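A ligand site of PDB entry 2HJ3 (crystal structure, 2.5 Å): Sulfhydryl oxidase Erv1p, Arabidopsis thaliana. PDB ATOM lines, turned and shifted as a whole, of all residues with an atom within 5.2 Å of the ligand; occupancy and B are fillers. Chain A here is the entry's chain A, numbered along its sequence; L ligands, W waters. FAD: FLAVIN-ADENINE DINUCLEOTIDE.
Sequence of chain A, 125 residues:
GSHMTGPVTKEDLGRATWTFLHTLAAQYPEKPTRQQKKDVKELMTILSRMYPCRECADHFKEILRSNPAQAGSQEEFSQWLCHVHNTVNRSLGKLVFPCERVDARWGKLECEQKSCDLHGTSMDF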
ATOM      1  N   LYS A  10      27.596   4.620  20.336  1.00  0.00           N
ATOM      2  CA  LYS A  10      26.152   4.767  20.271  1.00  0.00           C
ATOM      3  C   LYS A  10      25.504   3.752  21.227  1.00  0.00           C
ATOM      4  O   LYS A  10      24.498   4.048  21.870  1.00  0.00           O
ATOM      5  CB  LYS A  10      25.681   4.489  18.842  1.00  0.00           C
ATOM      6  CG  LYS A  10      24.182   4.407  18.681  1.00  0.00           C
ATOM      7  CD  LYS A  10      23.809   3.708  17.364  1.00  0.00           C
ATOM      8  CE  LYS A  10      24.290   4.494  16.143  1.00  0.00           C
ATOM      9  NZ  LYS A  10      23.814   3.878  14.872  1.00  0.00           N
ATOM     10  N   GLU A  11      26.108   2.571  21.325  1.00  0.00           N
ATOM     11  CA  GLU A  11      25.583   1.519  22.190  1.00  0.00           C
ATOM     12  C   GLU A  11      25.780   1.806  23.675  1.00  0.00           C
ATOM     13  O   GLU A  11      24.891   1.538  24.474  1.00  0.00           O
ATOM     14  CB  GLU A  11      26.208   0.170  21.846  1.00  0.00           C
ATOM     15  CG  GLU A  11      25.872  -0.362  20.443  1.00  0.00           C
ATOM     16  CD  GLU A  11      26.623   0.363  19.336  1.00  0.00           C
ATOM     17  OE1 GLU A  11      27.832   0.630  19.518  1.00  0.00           O
ATOM     18  OE2 GLU A  11      26.025   0.653  18.285  1.00  0.00           O
ATOM     19  N   LEU A  13      25.976   4.708  25.064  1.00  0.00           N
ATOM     20  CA  LEU A  13      25.068   5.799  25.393  1.00  0.00           C
ATOM     21  C   LEU A  13      23.684   5.219  25.631  1.00  0.00           C
ATOM     22  O   LEU A  13      23.057   5.482  26.656  1.00  0.00           O
ATOM     23  CB  LEU A  13      25.029   6.827  24.249  1.00  0.00           C
ATOM     24  CG  LEU A  13      24.196   8.083  24.499  1.00  0.00           C
ATOM     25  CD1 LEU A  13      24.853   8.910  25.577  1.00  0.00           C
ATOM     26  CD2 LEU A  13      24.061   8.905  23.218  1.00  0.00           C
ATOM     27  N   GLY A  14      23.224   4.418  24.669  1.00  0.00           N
ATOM     28  CA  GLY A  14      21.920   3.786  24.759  1.00  0.00           C
ATOM     29  C   GLY A  14      21.732   3.002  26.032  1.00  0.00           C
ATOM     30  O   GLY A  14      20.728   3.180  26.723  1.00  0.00           O
ATOM     31  N   ARG A  15      22.680   2.131  26.366  1.00  0.00           N
ATOM     32  CA  ARG A  15      22.579   1.320  27.582  1.00  0.00           C
ATOM     33  C   ARG A  15      22.529   2.148  28.852  1.00  0.00           C
ATOM     34  O   ARG A  15      21.794   1.829  29.780  1.00  0.00           O
ATOM     35  CB  ARG A  15      23.757   0.341  27.691  1.00  0.00           C
ATOM     36  CG  ARG A  15      23.623  -0.912  26.831  1.00  0.00           C
ATOM     37  CD  ARG A  15      24.738  -1.907  27.138  1.00  0.00           C
ATOM     38  NE  ARG A  15      26.010  -1.555  26.500  1.00  0.00           N
ATOM     39  CZ  ARG A  15      26.311  -1.829  25.232  1.00  0.00           C
ATOM     40  NH1 ARG A  15      25.438  -2.473  24.465  1.00  0.00           N
ATOM     41  NH2 ARG A  15      27.483  -1.451  24.734  1.00  0.00           N
ATOM     42  N   THR A  17      21.555   5.394  29.090  1.00  0.00           N
ATOM     43  CA  THR A  17      20.298   6.113  29.101  1.00  0.00           C
ATOM     44  C   THR A  17      19.102   5.228  29.466  1.00  0.00           C
ATOM     45  O   THR A  17      18.278   5.606  30.297  1.00  0.00           O
ATOM     46  CB  THR A  17      20.052   6.809  27.756  1.00  0.00           C
ATOM     47  OG1 THR A  17      21.153   7.673  27.454  1.00  0.00           O
ATOM     48  CG2 THR A  17      18.770   7.626  27.810  1.00  0.00           C
ATOM     49  N   TRP A  18      19.007   4.046  28.847  1.00  0.00           N
ATOM     50  CA  TRP A  18      17.890   3.155  29.178  1.00  0.00           C
ATOM     51  C   TRP A  18      17.902   2.837  30.678  1.00  0.00           C
ATOM     52  O   TRP A  18      16.855   2.878  31.337  1.00  0.00           O
ATOM     53  CB  TRP A  18      17.959   1.862  28.343  1.00  0.00           C
ATOM     54  CG  TRP A  18      17.592   2.043  26.886  1.00  0.00           C
ATOM     55  CD1 TRP A  18      18.345   1.698  25.806  1.00  0.00           C
ATOM     56  CD2 TRP A  18      16.389   2.636  26.371  1.00  0.00           C
ATOM     57  NE1 TRP A  18      17.685   2.032  24.636  1.00  0.00           N
ATOM     58  CE2 TRP A  18      16.490   2.615  24.958  1.00  0.00           C
ATOM     59  CE3 TRP A  18      15.239   3.191  26.967  1.00  0.00           C
ATOM     60  CZ2 TRP A  18      15.470   3.129  24.125  1.00  0.00           C
ATOM     61  CZ3 TRP A  18      14.230   3.701  26.124  1.00  0.00           C
ATOM     62  CH2 TRP A  18      14.357   3.660  24.726  1.00  0.00           C
ATOM     63  N   LEU A  21      16.549   5.891  32.352  1.00  0.00           N
ATOM     64  CA  LEU A  21      15.122   6.015  32.089  1.00  0.00           C
ATOM     65  C   LEU A  21      14.273   4.928  32.778  1.00  0.00           C
ATOM     66  O   LEU A  21      13.337   5.239  33.507  1.00  0.00           O
ATOM     67  CB  LEU A  21      14.854   6.033  30.588  1.00  0.00           C
ATOM     68  CG  LEU A  21      15.377   7.323  29.927  1.00  0.00           C
ATOM     69  CD1 LEU A  21      15.200   7.273  28.391  1.00  0.00           C
ATOM     70  CD2 LEU A  21      14.630   8.522  30.507  1.00  0.00           C
ATOM     71  N   HIS A  22      14.604   3.655  32.566  1.00  0.00           N
ATOM     72  CA  HIS A  22      13.824   2.599  33.204  1.00  0.00           C
ATOM     73  C   HIS A  22      13.944   2.646  34.726  1.00  0.00           C
ATOM     74  O   HIS A  22      12.982   2.353  35.429  1.00  0.00           O
ATOM     75  CB  HIS A  22      14.229   1.218  32.681  1.00  0.00           C
ATOM     76  CG  HIS A  22      13.885   1.013  31.230  1.00  0.00           C
ATOM     77  ND1 HIS A  22      12.592   1.093  30.754  1.00  0.00           N
ATOM     78  CD2 HIS A  22      14.667   0.766  30.153  1.00  0.00           C
ATOM     79  CE1 HIS A  22      12.600   0.910  29.451  1.00  0.00           C
ATOM     80  NE2 HIS A  22      13.844   0.717  29.056  1.00  0.00           N
ATOM     81  N   TYR A  51      18.923  14.120  22.684  1.00  0.00           N
ATOM     82  CA  TYR A  51      19.663  12.870  22.731  1.00  0.00           C
ATOM     83  C   TYR A  51      20.874  12.924  21.809  1.00  0.00           C
ATOM     84  O   TYR A  51      20.743  13.140  20.599  1.00  0.00           O
ATOM     85  CB  TYR A  51      18.760  11.691  22.361  1.00  0.00           C
ATOM     86  CG  TYR A  51      19.394  10.353  22.673  1.00  0.00           C
ATOM     87  CD1 TYR A  51      19.686   9.997  23.987  1.00  0.00           C
ATOM     88  CD2 TYR A  51      19.709   9.465  21.660  1.00  0.00           C
ATOM     89  CE1 TYR A  51      20.292   8.780  24.275  1.00  0.00           C
ATOM     90  CE2 TYR A  51      20.324   8.244  21.939  1.00  0.00           C
ATOM     91  CZ  TYR A  51      20.610   7.911  23.246  1.00  0.00           C
ATOM     92  OH  TYR A  51      21.233   6.712  23.532  1.00  0.00           O
ATOM     93  N   GLU A  55      20.450  10.288  14.525  1.00  0.00           N
ATOM     94  CA  GLU A  55      19.350   9.460  14.052  1.00  0.00           C
ATOM     95  C   GLU A  55      18.469   8.957  15.196  1.00  0.00           C
ATOM     96  O   GLU A  55      17.238   8.975  15.101  1.00  0.00           O
ATOM     97  CB  GLU A  55      19.886   8.246  13.284  1.00  0.00           C
ATOM     98  CG  GLU A  55      20.789   7.362  14.133  1.00  0.00           C
ATOM     99  CD  GLU A  55      20.961   5.978  13.555  1.00  0.00           C
ATOM    100  OE1 GLU A  55      21.433   5.863  12.406  1.00  0.00           O
ATOM    101  OE2 GLU A  55      20.629   4.992  14.266  1.00  0.00           O
ATOM    102  N   CYS A  56      19.107   8.504  16.271  1.00  0.00           N
ATOM    103  CA  CYS A  56      18.383   7.993  17.431  1.00  0.00           C
ATOM    104  C   CYS A  56      17.380   9.029  17.945  1.00  0.00           C
ATOM    105  O   CYS A  56      16.259   8.687  18.327  1.00  0.00           O
ATOM    106  CB  CYS A  56      19.333   7.667  18.572  1.00  0.00           C
ATOM    107  SG  CYS A  56      20.808   6.645  18.215  1.00  0.00           S
ATOM    108  N   HIS A  59      14.279   9.314  15.579  1.00  0.00           N
ATOM    109  CA  HIS A  59      13.363   8.193  15.778  1.00  0.00           C
ATOM    110  C   HIS A  59      12.552   8.361  17.045  1.00  0.00           C
ATOM    111  O   HIS A  59      11.340   8.127  17.048  1.00  0.00           O
ATOM    112  CB  HIS A  59      14.139   6.869  15.843  1.00  0.00           C
ATOM    113  CG  HIS A  59      14.692   6.443  14.522  1.00  0.00           C
ATOM    114  ND1 HIS A  59      15.519   5.346  14.381  1.00  0.00           N
ATOM    115  CD2 HIS A  59      14.533   6.951  13.280  1.00  0.00           C
ATOM    116  CE1 HIS A  59      15.847   5.200  13.120  1.00  0.00           C
ATOM    117  NE2 HIS A  59      15.265   6.160  12.425  1.00  0.00           N
ATOM    118  N   PHE A  60      13.221   8.772  18.110  1.00  0.00           N
ATOM    119  CA  PHE A  60      12.559   8.986  19.390  1.00  0.00           C
ATOM    120  C   PHE A  60      11.504  10.062  19.222  1.00  0.00           C
ATOM    121  O   PHE A  60      10.414   9.976  19.791  1.00  0.00           O
ATOM    122  CB  PHE A  60      13.575   9.398  20.468  1.00  0.00           C
ATOM    123  CG  PHE A  60      13.022   9.376  21.856  1.00  0.00           C
ATOM    124  CD1 PHE A  60      12.669   8.173  22.468  1.00  0.00           C
ATOM    125  CD2 PHE A  60      12.826  10.562  22.559  1.00  0.00           C
ATOM    126  CE1 PHE A  60      12.139   8.148  23.764  1.00  0.00           C
ATOM    127  CE2 PHE A  60      12.293  10.550  23.845  1.00  0.00           C
ATOM    128  CZ  PHE A  60      11.949   9.343  24.448  1.00  0.00           C
ATOM    129  N   LEU A  81       7.374   3.367  28.648  1.00  0.00           N
ATOM    130  CA  LEU A  81       8.817   3.405  28.389  1.00  0.00           C
ATOM    131  C   LEU A  81       9.312   2.085  27.811  1.00  0.00           C
ATOM    132  O   LEU A  81      10.234   2.054  27.009  1.00  0.00           O
ATOM    133  CB  LEU A  81       9.569   3.729  29.676  1.00  0.00           C
ATOM    134  CG  LEU A  81      11.009   4.248  29.535  1.00  0.00           C
ATOM    135  CD1 LEU A  81      11.066   5.422  28.569  1.00  0.00           C
ATOM    136  CD2 LEU A  81      11.514   4.652  30.895  1.00  0.00           C
ATOM    137  N   CYS A  82       8.683   0.986  28.219  1.00  0.00           N
ATOM    138  CA  CYS A  82       9.047  -0.341  27.724  1.00  0.00           C
ATOM    139  C   CYS A  82       8.600  -0.503  26.276  1.00  0.00           C
ATOM    140  O   CYS A  82       9.314  -1.103  25.459  1.00  0.00           O
ATOM    141  CB  CYS A  82       8.428  -1.427  28.595  1.00  0.00           C
ATOM    142  SG  CYS A  82       8.620  -3.129  27.987  1.00  0.00           S
ATOM    143  N   HIS A  83       7.425   0.041  25.953  1.00  0.00           N
ATOM    144  CA  HIS A  83       6.906  -0.054  24.590  1.00  0.00           C
ATOM    145  C   HIS A  83       7.765   0.777  23.661  1.00  0.00           C
ATOM    146  O   HIS A  83       8.045   0.394  22.519  1.00  0.00           O
ATOM    147  CB  HIS A  83       5.452   0.421  24.506  1.00  0.00           C
ATOM    148  CG  HIS A  83       4.496  -0.437  25.264  1.00  0.00           C
ATOM    149  ND1 HIS A  83       4.340  -1.780  25.003  1.00  0.00           N
ATOM    150  CD2 HIS A  83       3.711  -0.176  26.331  1.00  0.00           C
ATOM    151  CE1 HIS A  83       3.513  -2.315  25.886  1.00  0.00           C
ATOM    152  NE2 HIS A  83       3.103  -1.355  26.703  1.00  0.00           N
ATOM    153  N   HIS A  85      10.933   1.544  24.146  1.00  0.00           N
ATOM    154  CA  HIS A  85      12.187   0.824  23.984  1.00  0.00           C
ATOM    155  C   HIS A  85      12.020  -0.336  22.992  1.00  0.00           C
ATOM    156  O   HIS A  85      12.931  -0.628  22.219  1.00  0.00           O
ATOM    157  CB  HIS A  85      12.661   0.297  25.353  1.00  0.00           C
ATOM    158  CG  HIS A  85      14.086  -0.157  25.355  1.00  0.00           C
ATOM    159  ND1 HIS A  85      14.743  -0.505  26.528  1.00  0.00           N
ATOM    160  CD2 HIS A  85      14.989  -0.314  24.360  1.00  0.00           C
ATOM    161  CE1 HIS A  85      15.984  -0.838  26.240  1.00  0.00           C
ATOM    162  NE2 HIS A  85      16.165  -0.738  24.935  1.00  0.00           N
ATOM    163  N   ASN A  86      10.862  -0.988  22.996  1.00  0.00           N
ATOM    164  CA  ASN A  86      10.645  -2.099  22.068  1.00  0.00           C
ATOM    165  C   ASN A  86      10.580  -1.669  20.609  1.00  0.00           C
ATOM    166  O   ASN A  86      11.045  -2.383  19.721  1.00  0.00           O
ATOM    167  CB  ASN A  86       9.381  -2.885  22.432  1.00  0.00           C
ATOM    168  CG  ASN A  86       9.629  -3.880  23.529  1.00  0.00           C
ATOM    169  OD1 ASN A  86      10.715  -4.437  23.617  1.00  0.00           O
ATOM    170  ND2 ASN A  86       8.628  -4.129  24.354  1.00  0.00           N
ATOM    171  N   VAL A  88      12.275   0.587  19.305  1.00  0.00           N
ATOM    172  CA  VAL A  88      13.665   0.736  18.907  1.00  0.00           C
ATOM    173  C   VAL A  88      14.255  -0.660  18.720  1.00  0.00           C
ATOM    174  O   VAL A  88      14.898  -0.933  17.705  1.00  0.00           O
ATOM    175  CB  VAL A  88      14.484   1.528  19.953  1.00  0.00           C
ATOM    176  CG1 VAL A  88      15.935   1.609  19.522  1.00  0.00           C
ATOM    177  CG2 VAL A  88      13.900   2.937  20.108  1.00  0.00           C
ATOM    178  N   ASN A  89      14.016  -1.558  19.676  1.00  0.00           N
ATOM    179  CA  ASN A  89      14.509  -2.931  19.582  1.00  0.00           C
ATOM    180  C   ASN A  89      14.084  -3.579  18.261  1.00  0.00           C
ATOM    181  O   ASN A  89      14.905  -4.147  17.550  1.00  0.00           O
ATOM    182  CB  ASN A  89      13.987  -3.804  20.728  1.00  0.00           C
ATOM    183  CG  ASN A  89      14.637  -3.479  22.071  1.00  0.00           C
ATOM    184  OD1 ASN A  89      15.783  -3.020  22.127  1.00  0.00           O
ATOM    185  ND2 ASN A  89      13.925  -3.743  23.145  1.00  0.00           N
ATOM    186  N   LEU A  92      15.788  -2.404  15.149  1.00  0.00           N
ATOM    187  CA  LEU A  92      17.165  -2.857  15.101  1.00  0.00           C
ATOM    188  C   LEU A  92      17.323  -4.375  15.032  1.00  0.00           C
ATOM    189  O   LEU A  92      18.433  -4.887  15.113  1.00  0.00           O
ATOM    190  CB  LEU A  92      17.924  -2.348  16.318  1.00  0.00           C
ATOM    191  CG  LEU A  92      18.155  -0.842  16.417  1.00  0.00           C
ATOM    192  CD1 LEU A  92      18.906  -0.518  17.705  1.00  0.00           C
ATOM    193  CD2 LEU A  92      18.946  -0.385  15.192  1.00  0.00           C
ATOM    194  N   LYS A  94      16.341  -6.596  17.274  1.00  0.00           N
ATOM    195  CA  LYS A  94      16.717  -7.101  18.585  1.00  0.00           C
ATOM    196  C   LYS A  94      15.496  -7.723  19.247  1.00  0.00           C
ATOM    197  O   LYS A  94      14.359  -7.486  18.821  1.00  0.00           O
ATOM    198  CB  LYS A  94      17.243  -5.969  19.467  1.00  0.00           C
ATOM    199  CG  LYS A  94      18.616  -5.436  19.101  1.00  0.00           C
ATOM    200  CD  LYS A  94      18.981  -4.274  20.027  1.00  0.00           C
ATOM    201  CE  LYS A  94      20.464  -3.974  20.003  1.00  0.00           C
ATOM    202  NZ  LYS A  94      21.276  -5.122  20.512  1.00  0.00           N
ATOM    203  N   PHE A  97      11.168  -7.111  24.579  1.00  0.00           N
ATOM    204  CA  PHE A  97      10.947  -7.396  25.985  1.00  0.00           C
ATOM    205  C   PHE A  97       9.480  -7.413  26.379  1.00  0.00           C
ATOM    206  O   PHE A  97       8.715  -6.557  25.953  1.00  0.00           O
ATOM    207  CB  PHE A  97      11.711  -6.339  26.804  1.00  0.00           C
ATOM    208  CG  PHE A  97      11.730  -6.580  28.286  1.00  0.00           C
ATOM    209  CD1 PHE A  97      12.791  -7.257  28.865  1.00  0.00           C
ATOM    210  CD2 PHE A  97      10.707  -6.104  29.090  1.00  0.00           C
ATOM    211  CE1 PHE A  97      12.835  -7.457  30.256  1.00  0.00           C
ATOM    212  CE2 PHE A  97      10.734  -6.299  30.484  1.00  0.00           C
ATOM    213  CZ  PHE A  97      11.798  -6.962  31.060  1.00  0.00           C
ATOM    214  N   CYS A  99       6.709  -6.407  28.365  1.00  0.00           N
ATOM    215  CA  CYS A  99       6.479  -5.314  29.291  1.00  0.00           C
ATOM    216  C   CYS A  99       5.723  -5.612  30.572  1.00  0.00           C
ATOM    217  O   CYS A  99       5.404  -4.688  31.327  1.00  0.00           O
ATOM    218  CB  CYS A  99       5.810  -4.160  28.562  1.00  0.00           C
ATOM    219  SG  CYS A  99       6.795  -3.542  27.170  1.00  0.00           S
ATOM    220  N   VAL A 102       8.674  -5.613  33.244  1.00  0.00           N
ATOM    221  CA  VAL A 102       9.543  -4.454  33.481  1.00  0.00           C
ATOM    222  C   VAL A 102       9.851  -4.280  34.952  1.00  0.00           C
ATOM    223  O   VAL A 102      11.005  -4.078  35.322  1.00  0.00           O
ATOM    224  CB  VAL A 102       8.956  -3.099  32.986  1.00  0.00           C
ATOM    225  CG1 VAL A 102       9.550  -2.761  31.626  1.00  0.00           C
ATOM    226  CG2 VAL A 102       7.455  -3.157  32.939  1.00  0.00           C
ATOM    227  N   ARG A 105      12.477  -6.541  36.008  1.00  0.00           N
ATOM    228  CA  ARG A 105      13.790  -6.178  35.470  1.00  0.00           C
ATOM    229  C   ARG A 105      14.325  -4.880  36.088  1.00  0.00           C
ATOM    230  O   ARG A 105      15.544  -4.711  36.242  1.00  0.00           O
ATOM    231  CB  ARG A 105      13.707  -6.050  33.935  1.00  0.00           C
ATOM    232  CG  ARG A 105      14.960  -5.488  33.282  1.00  0.00           C
ATOM    233  CD  ARG A 105      16.137  -6.452  33.351  1.00  0.00           C
ATOM    234  NE  ARG A 105      17.385  -5.826  32.885  1.00  0.00           N
ATOM    235  CZ  ARG A 105      18.131  -5.004  33.629  1.00  0.00           C
ATOM    236  NH1 ARG A 105      17.772  -4.706  34.870  1.00  0.00           N
ATOM    237  NH2 ARG A 105      19.234  -4.477  33.117  1.00  0.00           N
ATOM    238  N   TRP A 106      13.424  -3.964  36.444  1.00  0.00           N
ATOM    239  CA  TRP A 106      13.827  -2.695  37.048  1.00  0.00           C
ATOM    240  C   TRP A 106      13.050  -2.447  38.342  1.00  0.00           C
ATOM    241  O   TRP A 106      11.864  -2.136  38.312  1.00  0.00           O
ATOM    242  CB  TRP A 106      13.594  -1.519  36.082  1.00  0.00           C
ATOM    243  CG  TRP A 106      14.164  -1.721  34.712  1.00  0.00           C
ATOM    244  CD1 TRP A 106      13.502  -2.166  33.597  1.00  0.00           C
ATOM    245  CD2 TRP A 106      15.538  -1.518  34.303  1.00  0.00           C
ATOM    246  NE1 TRP A 106      14.365  -2.245  32.532  1.00  0.00           N
ATOM    247  CE2 TRP A 106      15.621  -1.853  32.937  1.00  0.00           C
ATOM    248  CE3 TRP A 106      16.690  -1.075  34.962  1.00  0.00           C
ATOM    249  CZ2 TRP A 106      16.819  -1.762  32.209  1.00  0.00           C
ATOM    250  CZ3 TRP A 106      17.881  -0.988  34.239  1.00  0.00           C
ATOM    251  CH2 TRP A 106      17.931  -1.336  32.877  1.00  0.00           C
HETATM  252  PA  FAD L   1      19.416  -1.869  25.159  1.00  0.00           P
HETATM  253  O1A FAD L   1      18.355  -1.767  24.129  1.00  0.00           O
HETATM  254  O2A FAD L   1      20.485  -0.853  25.392  1.00  0.00           O
HETATM  255  O5B FAD L   1      19.245  -2.424  26.618  1.00  0.00           O
HETATM  256  C5B FAD L   1      19.188  -2.130  27.999  1.00  0.00           C
HETATM  257  C4B FAD L   1      19.053  -3.519  28.561  1.00  0.00           C
HETATM  258  O4B FAD L   1      17.812  -3.197  29.250  1.00  0.00           O
HETATM  259  C3B FAD L   1      18.864  -4.959  27.982  1.00  0.00           C
HETATM  260  O3B FAD L   1      20.083  -5.689  27.840  1.00  0.00           O
HETATM  261  C2B FAD L   1      17.805  -5.525  28.823  1.00  0.00           C
HETATM  262  O2B FAD L   1      18.221  -6.021  30.055  1.00  0.00           O
HETATM  263  C1B FAD L   1      16.915  -4.289  29.015  1.00  0.00           C
HETATM  264  N9A FAD L   1      15.788  -4.000  28.180  1.00  0.00           N
HETATM  265  C8A FAD L   1      15.506  -4.261  26.820  1.00  0.00           C
HETATM  266  N7A FAD L   1      14.351  -3.924  26.318  1.00  0.00           N
HETATM  267  C5A FAD L   1      13.710  -3.344  27.411  1.00  0.00           C
HETATM  268  C6A FAD L   1      12.431  -2.803  27.645  1.00  0.00           C
HETATM  269  N6A FAD L   1      11.538  -2.843  26.643  1.00  0.00           N
HETATM  270  N1A FAD L   1      12.137  -2.341  28.928  1.00  0.00           N
HETATM  271  C2A FAD L   1      12.970  -2.413  29.997  1.00  0.00           C
HETATM  272  N3A FAD L   1      14.262  -2.918  29.738  1.00  0.00           N
HETATM  273  C4A FAD L   1      14.564  -3.398  28.420  1.00  0.00           C
HETATM  274  N1  FAD L   1      20.237   3.017  18.350  1.00  0.00           N
HETATM  275  C2  FAD L   1      20.241   2.988  16.959  1.00  0.00           C
HETATM  276  O2  FAD L   1      21.094   2.356  16.299  1.00  0.00           O
HETATM  277  N3  FAD L   1      19.184   3.708  16.447  1.00  0.00           N
HETATM  278  C4  FAD L   1      18.200   4.381  17.207  1.00  0.00           C
HETATM  279  O4  FAD L   1      17.404   5.060  16.471  1.00  0.00           O
HETATM  280  C4X FAD L   1      18.240   4.360  18.595  1.00  0.00           C
HETATM  281  N5  FAD L   1      17.385   5.114  19.470  1.00  0.00           N
HETATM  282  C5X FAD L   1      17.489   5.244  20.871  1.00  0.00           C
HETATM  283  C6  FAD L   1      16.630   6.094  21.601  1.00  0.00           C
HETATM  284  C7  FAD L   1      16.818   6.239  23.006  1.00  0.00           C
HETATM  285  C7M FAD L   1      15.902   7.230  23.726  1.00  0.00           C
HETATM  286  C8  FAD L   1      17.828   5.504  23.701  1.00  0.00           C
HETATM  287  C8M FAD L   1      18.142   5.440  25.185  1.00  0.00           C
HETATM  288  C9  FAD L   1      18.676   4.672  22.940  1.00  0.00           C
HETATM  289  C9A FAD L   1      18.615   4.524  21.539  1.00  0.00           C
HETATM  290  N10 FAD L   1      19.372   3.712  20.548  1.00  0.00           N
HETATM  291  C10 FAD L   1      19.333   3.652  19.169  1.00  0.00           C
HETATM  292  C1' FAD L   1      20.246   2.736  21.101  1.00  0.00           C
HETATM  293  C2' FAD L   1      19.730   1.354  21.377  1.00  0.00           C
HETATM  294  O2' FAD L   1      18.308   1.405  21.688  1.00  0.00           O
HETATM  295  C3' FAD L   1      20.626   0.493  22.218  1.00  0.00           C
HETATM  296  O3' FAD L   1      20.652   1.042  23.529  1.00  0.00           O
HETATM  297  C4' FAD L   1      21.913  -0.197  21.818  1.00  0.00           C
HETATM  298  O4' FAD L   1      21.769  -0.743  20.481  1.00  0.00           O
HETATM  299  C5' FAD L   1      22.356  -1.339  22.640  1.00  0.00           C
HETATM  300  O5' FAD L   1      21.475  -2.468  22.707  1.00  0.00           O
HETATM  301  P   FAD L   1      21.581  -3.502  23.869  1.00  0.00           P
HETATM  302  O1P FAD L   1      21.218  -4.615  22.997  1.00  0.00           O
HETATM  303  O2P FAD L   1      22.817  -3.492  24.694  1.00  0.00           O
HETATM  304  O3P FAD L   1      20.260  -3.159  24.732  1.00  0.00           O
HETATM  305  O   HOH W   1      17.408  -1.255  21.619  1.00  0.00           O
HETATM  306  O   HOH W   2      17.516  -4.494  24.484  1.00  0.00           O
HETATM  307  O   HOH W   3      22.496   0.845  18.389  1.00  0.00           O
HETATM  308  O   HOH W   4      23.935  -3.192  20.365  1.00  0.00           O
HETATM  309  O   HOH W   5      22.235   5.549  21.337  1.00  0.00           O
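Residues that only touch the ligand: Gly 14 (3.3 Å), Thr 17 (3.5 Å), His 22 (3.3 Å), Tyr 51 (3.3 Å), Phe 60 (3.6 Å), Asn 86 (3.5 Å), Val 88 (3.2 Å), Leu 92 (3.7 Å), Phe 97 (3.5 Å) and Val 102 (3.8 Å). Within 4 Å of the ligand: Lys 10, Gly 14, Arg 15, Thr 17, Trp 18, His 22, Tyr 51, Glu 55, Cys 56, His 59, Phe 60, Cys 82, His 85, Asn 86, Val 88, Asn 89, Leu 92, Lys 94, Phe 97, Val 102, Arg 105 and Trp 106. The nearest printed residue that does not touch the ligand is Glu 11 (4.1 Å).
O1P of the ligand is in salt-bridge range of NZ of Lys 94. The indole nitrogen (NE1) of Trp 18 sits at hydrogen-bond distance from an oxygen (O2') of the ligand. NZ of Lys 10 lies close to O2 of the ligand, at 3.4 Å. The guanidinium group (NH1) of Arg 15 lies within salt-bridge range of an oxygen (O2P) of the ligand (2.8 Å). A nitrogen (N7A) of the ligand lies within hydrogen-bond range of the side-chain amide nitrogen (ND2) of Asn 89 (3.2 Å). The side-chain sulfur (SG) of Cys 56 sits close to a nitrogen (N3) of the ligand (3.8 Å). O1A of the ligand lies within hydrogen-bond range of NE2 of His 85, at 2.6 Å. A ring nitrogen (ND1) of His 59 is in hydrogen-bond range of an oxygen (O4) of the ligand (2.8 Å). O of Cys 82 is in hydrogen-bond range of N6A of the ligand (3.1 Å). A nitrogen (N3) of the ligand sits at hydrogen-bond distance from the side-chain carboxylate (OE2) of Glu 55 (2.9 Å). The guanidinium group (NE) of Arg 105 lies within hydrogen-bond range of an oxygen (O2B) of the ligand, 3.0 Å away. The indole nitrogen (NE1) of Trp 106 is in hydrogen-bond range of a nitrogen (N3A) of the ligand, at 2.9 Å. N6A of the ligand sits at hydrogen-bond distance from SG of Cys 82 (3.2 Å).
The backbone NH of Lys 94 lies within hydrogen-bond range of the backbone carbonyl oxygen of Asn 89. OH of Tyr 51 lies within hydrogen-bond range of N of Gly 14 (3.2 Å). The backbone carbonyl oxygen of Cys 82 lies within hydrogen-bond range of the side-chain amide nitrogen of Asn 86 (3.3 Å). NE1 of Trp 18 is in hydrogen-bond range of NE2 of His 85, 3.2 Å away. The side-chain carboxylate of Glu 55 is in salt-bridge range of the side-chain amino group of Lys 10, at 3.4 Å. The side-chain amide oxygen (OD1) of Asn 86 sits at hydrogen-bond distance from the side-chain amide nitrogen (ND2) of Asn 89 (3.3 Å). A ring nitrogen (NE2) of His 22 sits at hydrogen-bond distance from a ring nitrogen (ND1) of His 85 (2.9 Å). O of Leu 13 sits at hydrogen-bond distance from OG1 of Thr 17 (3.0 Å).
Water W1 bridges OD1 of Asn 89 and O1A of the ligand. Water W2 bridges an oxygen (O1A) of the ligand and the side-chain amide oxygen (OD1) of Asn 89. Water W4 bridges O4' of the ligand and NZ of Lys 94. Water W5 lies within hydrogen-bond range of OH of Tyr 51, O of Lys 10 and SG of Cys 56.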
